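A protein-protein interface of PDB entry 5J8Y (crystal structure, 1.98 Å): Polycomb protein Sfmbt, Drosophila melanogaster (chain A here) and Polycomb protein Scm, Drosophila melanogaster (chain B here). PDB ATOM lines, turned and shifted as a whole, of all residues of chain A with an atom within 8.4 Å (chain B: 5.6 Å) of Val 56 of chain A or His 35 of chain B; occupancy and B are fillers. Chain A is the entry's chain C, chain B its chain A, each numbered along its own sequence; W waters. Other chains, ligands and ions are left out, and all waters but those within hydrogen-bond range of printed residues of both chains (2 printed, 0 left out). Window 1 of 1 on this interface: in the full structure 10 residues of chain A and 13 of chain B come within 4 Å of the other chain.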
ATOM      1  N   LYS A  45      -3.534 -10.032  29.146  1.00  0.00           N
ATOM      2  CA  LYS A  45      -3.822  -8.606  29.096  1.00  0.00           C
ATOM      3  C   LYS A  45      -5.329  -8.380  29.150  1.00  0.00           C
ATOM      4  O   LYS A  45      -5.801  -7.470  29.830  1.00  0.00           O
ATOM      5  CB  LYS A  45      -3.232  -7.974  27.838  1.00  0.00           C
ATOM      6  CG  LYS A  45      -1.714  -7.972  27.802  1.00  0.00           C
ATOM      7  CD  LYS A  45      -1.209  -7.467  26.460  1.00  0.00           C
ATOM      8  CE  LYS A  45       0.136  -8.076  26.096  1.00  0.00           C
ATOM      9  NZ  LYS A  45       1.263  -7.465  26.855  1.00  0.00           N
ATOM     10  N   ILE A  48      -6.128  -8.344  32.589  1.00  0.00           N
ATOM     11  CA  ILE A  48      -5.506  -7.236  33.302  1.00  0.00           C
ATOM     12  C   ILE A  48      -6.225  -5.911  33.039  1.00  0.00           C
ATOM     13  O   ILE A  48      -6.200  -5.015  33.882  1.00  0.00           O
ATOM     14  CB  ILE A  48      -4.009  -7.124  32.912  1.00  0.00           C
ATOM     15  CG1 ILE A  48      -3.225  -8.263  33.570  1.00  0.00           C
ATOM     16  CG2 ILE A  48      -3.408  -5.782  33.329  1.00  0.00           C
ATOM     17  CD1 ILE A  48      -1.842  -8.484  32.997  1.00  0.00           C
ATOM     18  N   MET A  49      -6.886  -5.828  31.894  1.00  0.00           N
ATOM     19  CA  MET A  49      -7.515  -4.584  31.461  1.00  0.00           C
ATOM     20  C   MET A  49      -8.603  -4.125  32.453  1.00  0.00           C
ATOM     21  O   MET A  49      -8.508  -3.052  32.985  1.00  0.00           O
ATOM     22  CB  MET A  49      -8.061  -4.701  30.059  1.00  0.00           C
ATOM     23  CG  MET A  49      -7.041  -4.486  28.965  1.00  0.00           C
ATOM     24  SD  MET A  49      -6.124  -2.940  29.049  1.00  0.00           S
ATOM     25  CE  MET A  49      -7.435  -1.746  28.879  1.00  0.00           C
ATOM     26  N   LEU A  52      -7.585  -2.953  35.976  1.00  0.00           N
ATOM     27  CA  LEU A  52      -6.970  -1.633  36.077  1.00  0.00           C
ATOM     28  C   LEU A  52      -7.835  -0.555  35.430  1.00  0.00           C
ATOM     29  O   LEU A  52      -7.324   0.434  34.909  1.00  0.00           O
ATOM     30  CB  LEU A  52      -5.583  -1.648  35.434  1.00  0.00           C
ATOM     31  CG  LEU A  52      -4.577  -2.646  36.014  1.00  0.00           C
ATOM     32  CD1 LEU A  52      -3.257  -2.476  35.319  1.00  0.00           C
ATOM     33  CD2 LEU A  52      -4.398  -2.469  37.507  1.00  0.00           C
ATOM     34  N   GLY A  53      -9.149  -0.756  35.467  1.00  0.00           N
ATOM     35  CA  GLY A  53     -10.092   0.249  35.010  1.00  0.00           C
ATOM     36  C   GLY A  53     -10.035   0.505  33.517  1.00  0.00           C
ATOM     37  O   GLY A  53     -10.263   1.628  33.065  1.00  0.00           O
ATOM     38  N   MET A  54      -9.731  -0.535  32.755  1.00  0.00           N
ATOM     39  CA  MET A  54      -9.686  -0.453  31.314  1.00  0.00           C
ATOM     40  C   MET A  54      -8.670   0.591  30.833  1.00  0.00           C
ATOM     41  O   MET A  54      -8.864   1.228  29.829  1.00  0.00           O
ATOM     42  CB  MET A  54     -11.072  -0.155  30.736  1.00  0.00           C
ATOM     43  CG  MET A  54     -12.130  -1.219  31.022  1.00  0.00           C
ATOM     44  SD  MET A  54     -11.647  -2.916  30.681  1.00  0.00           S
ATOM     45  CE  MET A  54     -11.654  -2.893  28.901  1.00  0.00           C
ATOM     46  N   LYS A  55      -7.589   0.750  31.566  1.00  0.00           N
ATOM     47  CA  LYS A  55      -6.520   1.675  31.198  1.00  0.00           C
ATOM     48  C   LYS A  55      -5.338   0.919  30.595  1.00  0.00           C
ATOM     49  O   LYS A  55      -4.752   0.052  31.241  1.00  0.00           O
ATOM     50  CB  LYS A  55      -6.067   2.481  32.416  1.00  0.00           C
ATOM     51  CG  LYS A  55      -7.118   3.447  32.937  1.00  0.00           C
ATOM     52  CD  LYS A  55      -6.685   4.095  34.241  1.00  0.00           C
ATOM     53  CE  LYS A  55      -7.423   5.402  34.476  1.00  0.00           C
ATOM     54  NZ  LYS A  55      -7.412   5.802  35.908  1.00  0.00           N
ATOM     55  N   VAL A  56      -5.014   1.243  29.355  1.00  0.00           N
ATOM     56  CA  VAL A  56      -3.979   0.551  28.606  1.00  0.00           C
ATOM     57  C   VAL A  56      -2.571   0.733  29.192  1.00  0.00           C
ATOM     58  O   VAL A  56      -1.820  -0.206  29.281  1.00  0.00           O
ATOM     59  CB  VAL A  56      -3.992   0.980  27.120  1.00  0.00           C
ATOM     60  CG1 VAL A  56      -2.760   0.491  26.362  1.00  0.00           C
ATOM     61  CG2 VAL A  56      -5.238   0.462  26.462  1.00  0.00           C
ATOM     62  N   GLY A  57      -2.228   1.963  29.535  1.00  0.00           N
ATOM     63  CA  GLY A  57      -0.903   2.271  30.048  1.00  0.00           C
ATOM     64  C   GLY A  57      -0.513   1.399  31.229  1.00  0.00           C
ATOM     65  O   GLY A  57       0.476   0.669  31.163  1.00  0.00           O
ATOM     66  N   PRO A  58      -1.286   1.478  32.321  1.00  0.00           N
ATOM     67  CA  PRO A  58      -1.083   0.624  33.498  1.00  0.00           C
ATOM     68  C   PRO A  58      -1.144  -0.866  33.161  1.00  0.00           C
ATOM     69  O   PRO A  58      -0.340  -1.646  33.668  1.00  0.00           O
ATOM     70  CB  PRO A  58      -2.236   1.021  34.424  1.00  0.00           C
ATOM     71  CG  PRO A  58      -2.594   2.402  34.018  1.00  0.00           C
ATOM     72  CD  PRO A  58      -2.335   2.488  32.545  1.00  0.00           C
ATOM     73  N   ALA A  59      -2.100  -1.243  32.317  1.00  0.00           N
ATOM     74  CA  ALA A  59      -2.264  -2.631  31.894  1.00  0.00           C
ATOM     75  C   ALA A  59      -0.997  -3.184  31.250  1.00  0.00           C
ATOM     76  O   ALA A  59      -0.578  -4.301  31.553  1.00  0.00           O
ATOM     77  CB  ALA A  59      -3.433  -2.749  30.932  1.00  0.00           C
ATOM     78  N   LEU A  60      -0.405  -2.406  30.378  1.00  0.00           N
ATOM     79  CA  LEU A  60       0.793  -2.807  29.707  1.00  0.00           C
ATOM     80  C   LEU A  60       1.981  -2.882  30.657  1.00  0.00           C
ATOM     81  O   LEU A  60       2.797  -3.730  30.563  1.00  0.00           O
ATOM     82  CB  LEU A  60       1.078  -1.921  28.551  1.00  0.00           C
ATOM     83  CG  LEU A  60       0.417  -2.322  27.242  1.00  0.00           C
ATOM     84  CD1 LEU A  60       0.493  -1.188  26.278  1.00  0.00           C
ATOM     85  CD2 LEU A  60       0.897  -3.621  26.613  1.00  0.00           C
ATOM     86  N   LYS A  61       2.028  -1.958  31.573  1.00  0.00           N
ATOM     87  CA  LYS A  61       3.082  -1.893  32.537  1.00  0.00           C
ATOM     88  C   LYS A  61       3.062  -3.105  33.450  1.00  0.00           C
ATOM     89  O   LYS A  61       4.070  -3.672  33.722  1.00  0.00           O
ATOM     90  CB  LYS A  61       3.029  -0.611  33.319  1.00  0.00           C
ATOM     91  CG  LYS A  61       3.776   0.559  32.704  1.00  0.00           C
ATOM     92  CD  LYS A  61       3.382   1.839  33.413  1.00  0.00           C
ATOM     93  CE  LYS A  61       4.025   3.080  32.903  1.00  0.00           C
ATOM     94  NZ  LYS A  61       3.438   4.246  33.528  1.00  0.00           N
ATOM     95  N   ILE A  62       1.882  -3.495  33.886  1.00  0.00           N
ATOM     96  CA  ILE A  62       1.695  -4.670  34.730  1.00  0.00           C
ATOM     97  C   ILE A  62       1.986  -5.948  33.947  1.00  0.00           C
ATOM     98  O   ILE A  62       2.623  -6.862  34.467  1.00  0.00           O
ATOM     99  CB  ILE A  62       0.259  -4.723  35.310  1.00  0.00           C
ATOM    100  CG1 ILE A  62       0.063  -3.625  36.362  1.00  0.00           C
ATOM    101  CG2 ILE A  62      -0.046  -6.088  35.923  1.00  0.00           C
ATOM    102  CD1 ILE A  62       0.946  -3.751  37.591  1.00  0.00           C
ATOM    103  N   SER A  63       1.516  -6.017  32.704  1.00  0.00           N
ATOM    104  CA  SER A  63       1.800  -7.173  31.858  1.00  0.00           C
ATOM    105  C   SER A  63       3.307  -7.350  31.706  1.00  0.00           C
ATOM    106  O   SER A  63       3.824  -8.463  31.804  1.00  0.00           O
ATOM    107  CB  SER A  63       1.147  -7.021  30.484  1.00  0.00           C
ATOM    108  OG  SER A  63       1.426  -8.145  29.664  1.00  0.00           O
ATOM    109  N   ASP B  30      -6.707  13.745  24.973  1.00  0.00           N
ATOM    110  CA  ASP B  30      -7.428  13.259  26.148  1.00  0.00           C
ATOM    111  C   ASP B  30      -7.477  11.735  26.221  1.00  0.00           C
ATOM    112  O   ASP B  30      -7.604  11.164  27.306  1.00  0.00           O
ATOM    113  CB  ASP B  30      -8.855  13.817  26.166  1.00  0.00           C
ATOM    114  CG  ASP B  30      -8.903  15.294  26.512  1.00  0.00           C
ATOM    115  OD1 ASP B  30      -7.927  15.804  27.103  1.00  0.00           O
ATOM    116  OD2 ASP B  30      -9.921  15.946  26.200  1.00  0.00           O
ATOM    117  N   LEU B  31      -7.376  11.089  25.088  1.00  0.00           N
ATOM    118  CA  LEU B  31      -7.391   9.642  25.027  1.00  0.00           C
ATOM    119  C   LEU B  31      -6.124   9.087  25.711  1.00  0.00           C
ATOM    120  O   LEU B  31      -6.179   8.172  26.463  1.00  0.00           O
ATOM    121  CB  LEU B  31      -7.489   9.158  23.598  1.00  0.00           C
ATOM    122  CG  LEU B  31      -7.640   7.665  23.472  1.00  0.00           C
ATOM    123  CD1 LEU B  31      -8.973   7.212  23.993  1.00  0.00           C
ATOM    124  CD2 LEU B  31      -7.402   7.197  22.075  1.00  0.00           C
ATOM    125  N   PHE B  32      -5.001   9.713  25.427  1.00  0.00           N
ATOM    126  CA  PHE B  32      -3.721   9.350  26.001  1.00  0.00           C
ATOM    127  C   PHE B  32      -3.679   9.620  27.486  1.00  0.00           C
ATOM    128  O   PHE B  32      -3.052   8.931  28.206  1.00  0.00           O
ATOM    129  CB  PHE B  32      -2.606  10.055  25.293  1.00  0.00           C
ATOM    130  CG  PHE B  32      -2.158   9.347  24.085  1.00  0.00           C
ATOM    131  CD1 PHE B  32      -3.000   9.151  23.040  1.00  0.00           C
ATOM    132  CD2 PHE B  32      -0.917   8.868  24.000  1.00  0.00           C
ATOM    133  CE1 PHE B  32      -2.588   8.503  21.928  1.00  0.00           C
ATOM    134  CE2 PHE B  32      -0.504   8.205  22.892  1.00  0.00           C
ATOM    135  CZ  PHE B  32      -1.346   8.030  21.859  1.00  0.00           C
ATOM    136  N   ARG B  33      -4.383  10.658  27.915  1.00  0.00           N
ATOM    137  CA  ARG B  33      -4.461  11.006  29.313  1.00  0.00           C
ATOM    138  C   ARG B  33      -5.277   9.966  30.070  1.00  0.00           C
ATOM    139  O   ARG B  33      -4.860   9.495  31.094  1.00  0.00           O
ATOM    140  CB  ARG B  33      -5.034  12.423  29.491  1.00  0.00           C
ATOM    141  CG  ARG B  33      -4.261  13.502  28.770  1.00  0.00           C
ATOM    142  CD  ARG B  33      -4.813  14.921  28.937  1.00  0.00           C
ATOM    143  NE  ARG B  33      -3.894  15.880  28.384  1.00  0.00           N
ATOM    144  CZ  ARG B  33      -3.992  16.408  27.169  1.00  0.00           C
ATOM    145  NH1 ARG B  33      -5.004  16.106  26.371  1.00  0.00           N
ATOM    146  NH2 ARG B  33      -3.085  17.252  26.756  1.00  0.00           N
ATOM    147  N   LYS B  34      -6.428   9.593  29.523  1.00  0.00           N
ATOM    148  CA  LYS B  34      -7.280   8.594  30.166  1.00  0.00           C
ATOM    149  C   LYS B  34      -6.527   7.292  30.393  1.00  0.00           C
ATOM    150  O   LYS B  34      -6.579   6.712  31.479  1.00  0.00           O
ATOM    151  CB  LYS B  34      -8.534   8.310  29.334  1.00  0.00           C
ATOM    152  CG  LYS B  34      -9.252   7.029  29.767  1.00  0.00           C
ATOM    153  CD  LYS B  34     -10.704   6.976  29.318  1.00  0.00           C
ATOM    154  CE  LYS B  34     -11.493   5.946  30.127  1.00  0.00           C
ATOM    155  NZ  LYS B  34     -11.239   4.536  29.702  1.00  0.00           N
ATOM    156  N   HIS B  35      -5.811   6.845  29.368  1.00  0.00           N
ATOM    157  CA  HIS B  35      -5.086   5.581  29.403  1.00  0.00           C
ATOM    158  C   HIS B  35      -3.729   5.707  30.071  1.00  0.00           C
ATOM    159  O   HIS B  35      -2.997   4.737  30.230  1.00  0.00           O
ATOM    160  CB  HIS B  35      -4.964   4.995  27.999  1.00  0.00           C
ATOM    161  CG  HIS B  35      -6.270   4.558  27.440  1.00  0.00           C
ATOM    162  ND1 HIS B  35      -6.866   3.379  27.805  1.00  0.00           N
ATOM    163  CD2 HIS B  35      -7.146   5.187  26.631  1.00  0.00           C
ATOM    164  CE1 HIS B  35      -8.035   3.280  27.208  1.00  0.00           C
ATOM    165  NE2 HIS B  35      -8.226   4.360  26.488  1.00  0.00           N
ATOM    166  N   GLU B  36      -3.432   6.923  30.481  1.00  0.00           N
ATOM    167  CA  GLU B  36      -2.197   7.200  31.209  1.00  0.00           C
ATOM    168  C   GLU B  36      -0.982   6.707  30.430  1.00  0.00           C
ATOM    169  O   GLU B  36      -0.138   5.979  30.956  1.00  0.00           O
ATOM    170  CB  GLU B  36      -2.248   6.560  32.600  1.00  0.00           C
ATOM    171  CG  GLU B  36      -3.328   7.156  33.499  1.00  0.00           C
ATOM    172  CD  GLU B  36      -3.391   6.507  34.870  1.00  0.00           C
ATOM    173  OE1 GLU B  36      -2.561   5.617  35.154  1.00  0.00           O
ATOM    174  OE2 GLU B  36      -4.275   6.891  35.665  1.00  0.00           O
ATOM    175  N   ILE B  37      -0.907   7.112  29.168  1.00  0.00           N
ATOM    176  CA  ILE B  37       0.199   6.724  28.309  1.00  0.00           C
ATOM    177  C   ILE B  37       1.350   7.713  28.449  1.00  0.00           C
ATOM    178  O   ILE B  37       1.401   8.729  27.753  1.00  0.00           O
ATOM    179  CB  ILE B  37      -0.239   6.633  26.829  1.00  0.00           C
ATOM    180  CG1 ILE B  37      -1.402   5.646  26.663  1.00  0.00           C
ATOM    181  CG2 ILE B  37       0.927   6.226  25.941  1.00  0.00           C
ATOM    182  CD1 ILE B  37      -1.187   4.284  27.322  1.00  0.00           C
ATOM    183  N   LEU B  45       3.425  -0.028  23.811  1.00  0.00           N
ATOM    184  CA  LEU B  45       2.234  -0.168  22.977  1.00  0.00           C
ATOM    185  C   LEU B  45       2.443  -1.123  21.808  1.00  0.00           C
ATOM    186  O   LEU B  45       3.571  -1.421  21.417  1.00  0.00           O
ATOM    187  CB  LEU B  45       1.797   1.191  22.430  1.00  0.00           C
ATOM    188  CG  LEU B  45       0.889   2.039  23.317  1.00  0.00           C
ATOM    189  CD1 LEU B  45       0.874   3.461  22.819  1.00  0.00           C
ATOM    190  CD2 LEU B  45      -0.518   1.469  23.338  1.00  0.00           C
ATOM    191  N   MET B  49      -3.379  -3.333  21.046  1.00  0.00           N
ATOM    192  CA  MET B  49      -3.871  -2.631  22.231  1.00  0.00           C
ATOM    193  C   MET B  49      -4.474  -1.278  21.855  1.00  0.00           C
ATOM    194  O   MET B  49      -5.440  -0.826  22.471  1.00  0.00           O
ATOM    195  CB  MET B  49      -2.745  -2.436  23.250  1.00  0.00           C
ATOM    196  CG  MET B  49      -2.190  -3.733  23.828  1.00  0.00           C
ATOM    197  SD  MET B  49      -3.401  -4.679  24.770  1.00  0.00           S
ATOM    198  CE  MET B  49      -3.564  -3.663  26.236  1.00  0.00           C
ATOM    199  N   TYR B  53      -8.404  -1.569  22.573  1.00  0.00           N
ATOM    200  CA  TYR B  53      -8.683  -1.003  23.882  1.00  0.00           C
ATOM    201  C   TYR B  53      -8.643   0.532  23.990  1.00  0.00           C
ATOM    202  O   TYR B  53      -9.181   1.105  24.913  1.00  0.00           O
ATOM    203  CB  TYR B  53      -7.762  -1.665  24.885  1.00  0.00           C
ATOM    204  CG  TYR B  53      -8.188  -3.076  25.199  1.00  0.00           C
ATOM    205  CD1 TYR B  53      -9.475  -3.338  25.626  1.00  0.00           C
ATOM    206  CD2 TYR B  53      -7.330  -4.143  25.035  1.00  0.00           C
ATOM    207  CE1 TYR B  53      -9.893  -4.613  25.905  1.00  0.00           C
ATOM    208  CE2 TYR B  53      -7.737  -5.435  25.295  1.00  0.00           C
ATOM    209  CZ  TYR B  53      -9.027  -5.670  25.731  1.00  0.00           C
ATOM    210  OH  TYR B  53      -9.440  -6.945  26.001  1.00  0.00           O
ATOM    211  N   MET B  54      -8.050   1.199  23.016  1.00  0.00           N
ATOM    212  CA  MET B  54      -8.039   2.662  23.007  1.00  0.00           C
ATOM    213  C   MET B  54      -9.026   3.198  21.971  1.00  0.00           C
ATOM    214  O   MET B  54      -9.331   4.389  21.953  1.00  0.00           O
ATOM    215  CB  MET B  54      -6.630   3.198  22.740  1.00  0.00           C
ATOM    216  CG  MET B  54      -5.609   2.763  23.776  1.00  0.00           C
ATOM    217  SD  MET B  54      -3.963   3.466  23.541  1.00  0.00           S
ATOM    218  CE  MET B  54      -4.270   5.205  23.862  1.00  0.00           C
HETATM  219  O   HOH W   1      -9.944   0.053  27.106  1.00  0.00           O
HETATM  220  O   HOH W   2       0.782   4.213  32.883  1.00  0.00           O
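The backbone NH of Ile 37 of chain B lies within hydrogen-bond range of the backbone carbonyl oxygen of Phe 32 of chain B (3.0 Å).
O of Met 49 of chain B lies within hydrogen-bond range of N of Met 54 of chain B.
The side-chain hydroxyl of Ser 63 of chain A is in hydrogen-bond range of the side-chain amino group of Lys 45 of chain A, at 2.9 Å.
O of Met 49 of chain A sits at hydrogen-bond distance from N of Met 54 of chain A, 2.8 Å away.
A ring nitrogen (ND1) of His 35 of chain B sits at hydrogen-bond distance from the backbone NH of Val 56 of chain A, 3.2 Å away.
The backbone NH of Gly 57 of chain A is in hydrogen-bond range of the backbone carbonyl oxygen of His 35 of chain B (3.0 Å).
OE2 of Glu 36 of chain B is in salt-bridge range of NZ of Lys 55 of chain A, at 3.3 Å.
Water W1 bridges O of Tyr 53 of chain B and O of Met 54 of chain A.
Water W2 lies within hydrogen-bond range of the side-chain amino group (NZ) of Lys 61 of chain A (2.7 Å) and the backbone carbonyl oxygen (O) of Glu 36 of chain B (2.8 Å).
Ile 48 of chain A touches none of the printed residues of chain B.
Printed residues of chain B within 4 Å of Met 54 of chain A: His 35 and Tyr 53.
Leu 31 of chain B touches none of the printed residues of chain A.
Of the printed residues of chain A, Tyr 53 of chain B touches Met 49, Met 54 and Val 56.
Of the printed residues of chain A, Met 54 of chain B touches Val 56 (3.6 Å).
Hydrophobic or aromatic side chains of chain A within 4 Å of the printed part of chain B: Met 49, Met 54, Val 56, Pro 58 and Leu 60.
Of the 12 printed residues of chain B, 8 touch a printed residue of chain A.
Printed residues of chain B that touch a printed residue of chain A: Lys 34, His 35, Glu 36, Ile 37, Leu 45, Met 49, Tyr 53 and Met 54.
Among the printed residues, Asp or Glu carboxylates within 4 Å of a Lys or Arg side-chain nitrogen of the other chain: Lys 55 of chain A with Glu 36 of chain B.
Tyr 53 of chain B touches Met 49 of chain A.
CE1 of Tyr 53 of chain B touches CE of Met 54 of chain A, 3.9 Å away.
Lys 55 of chain A touches Lys 34 of chain B.
Leu 45 of chain B touches Val 56 of chain A (CD2 to CG1, 3.9 Å).
Val 56 of chain A touches Tyr 53 of chain B.
Met 54 of chain B touches Val 56 of chain A.
N of Gly 57 of chain A touches CD1 of Ile 37 of chain B, at 3.4 Å.
O of His 35 of chain B touches CD of Pro 58 of chain A, at 3.3 Å.
Pro 58 of chain A touches Glu 36 of chain B (CG to OE1, 3.4 Å).
CD1 of Leu 60 of chain A touches CA of Leu 45 of chain B, at 3.9 Å.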
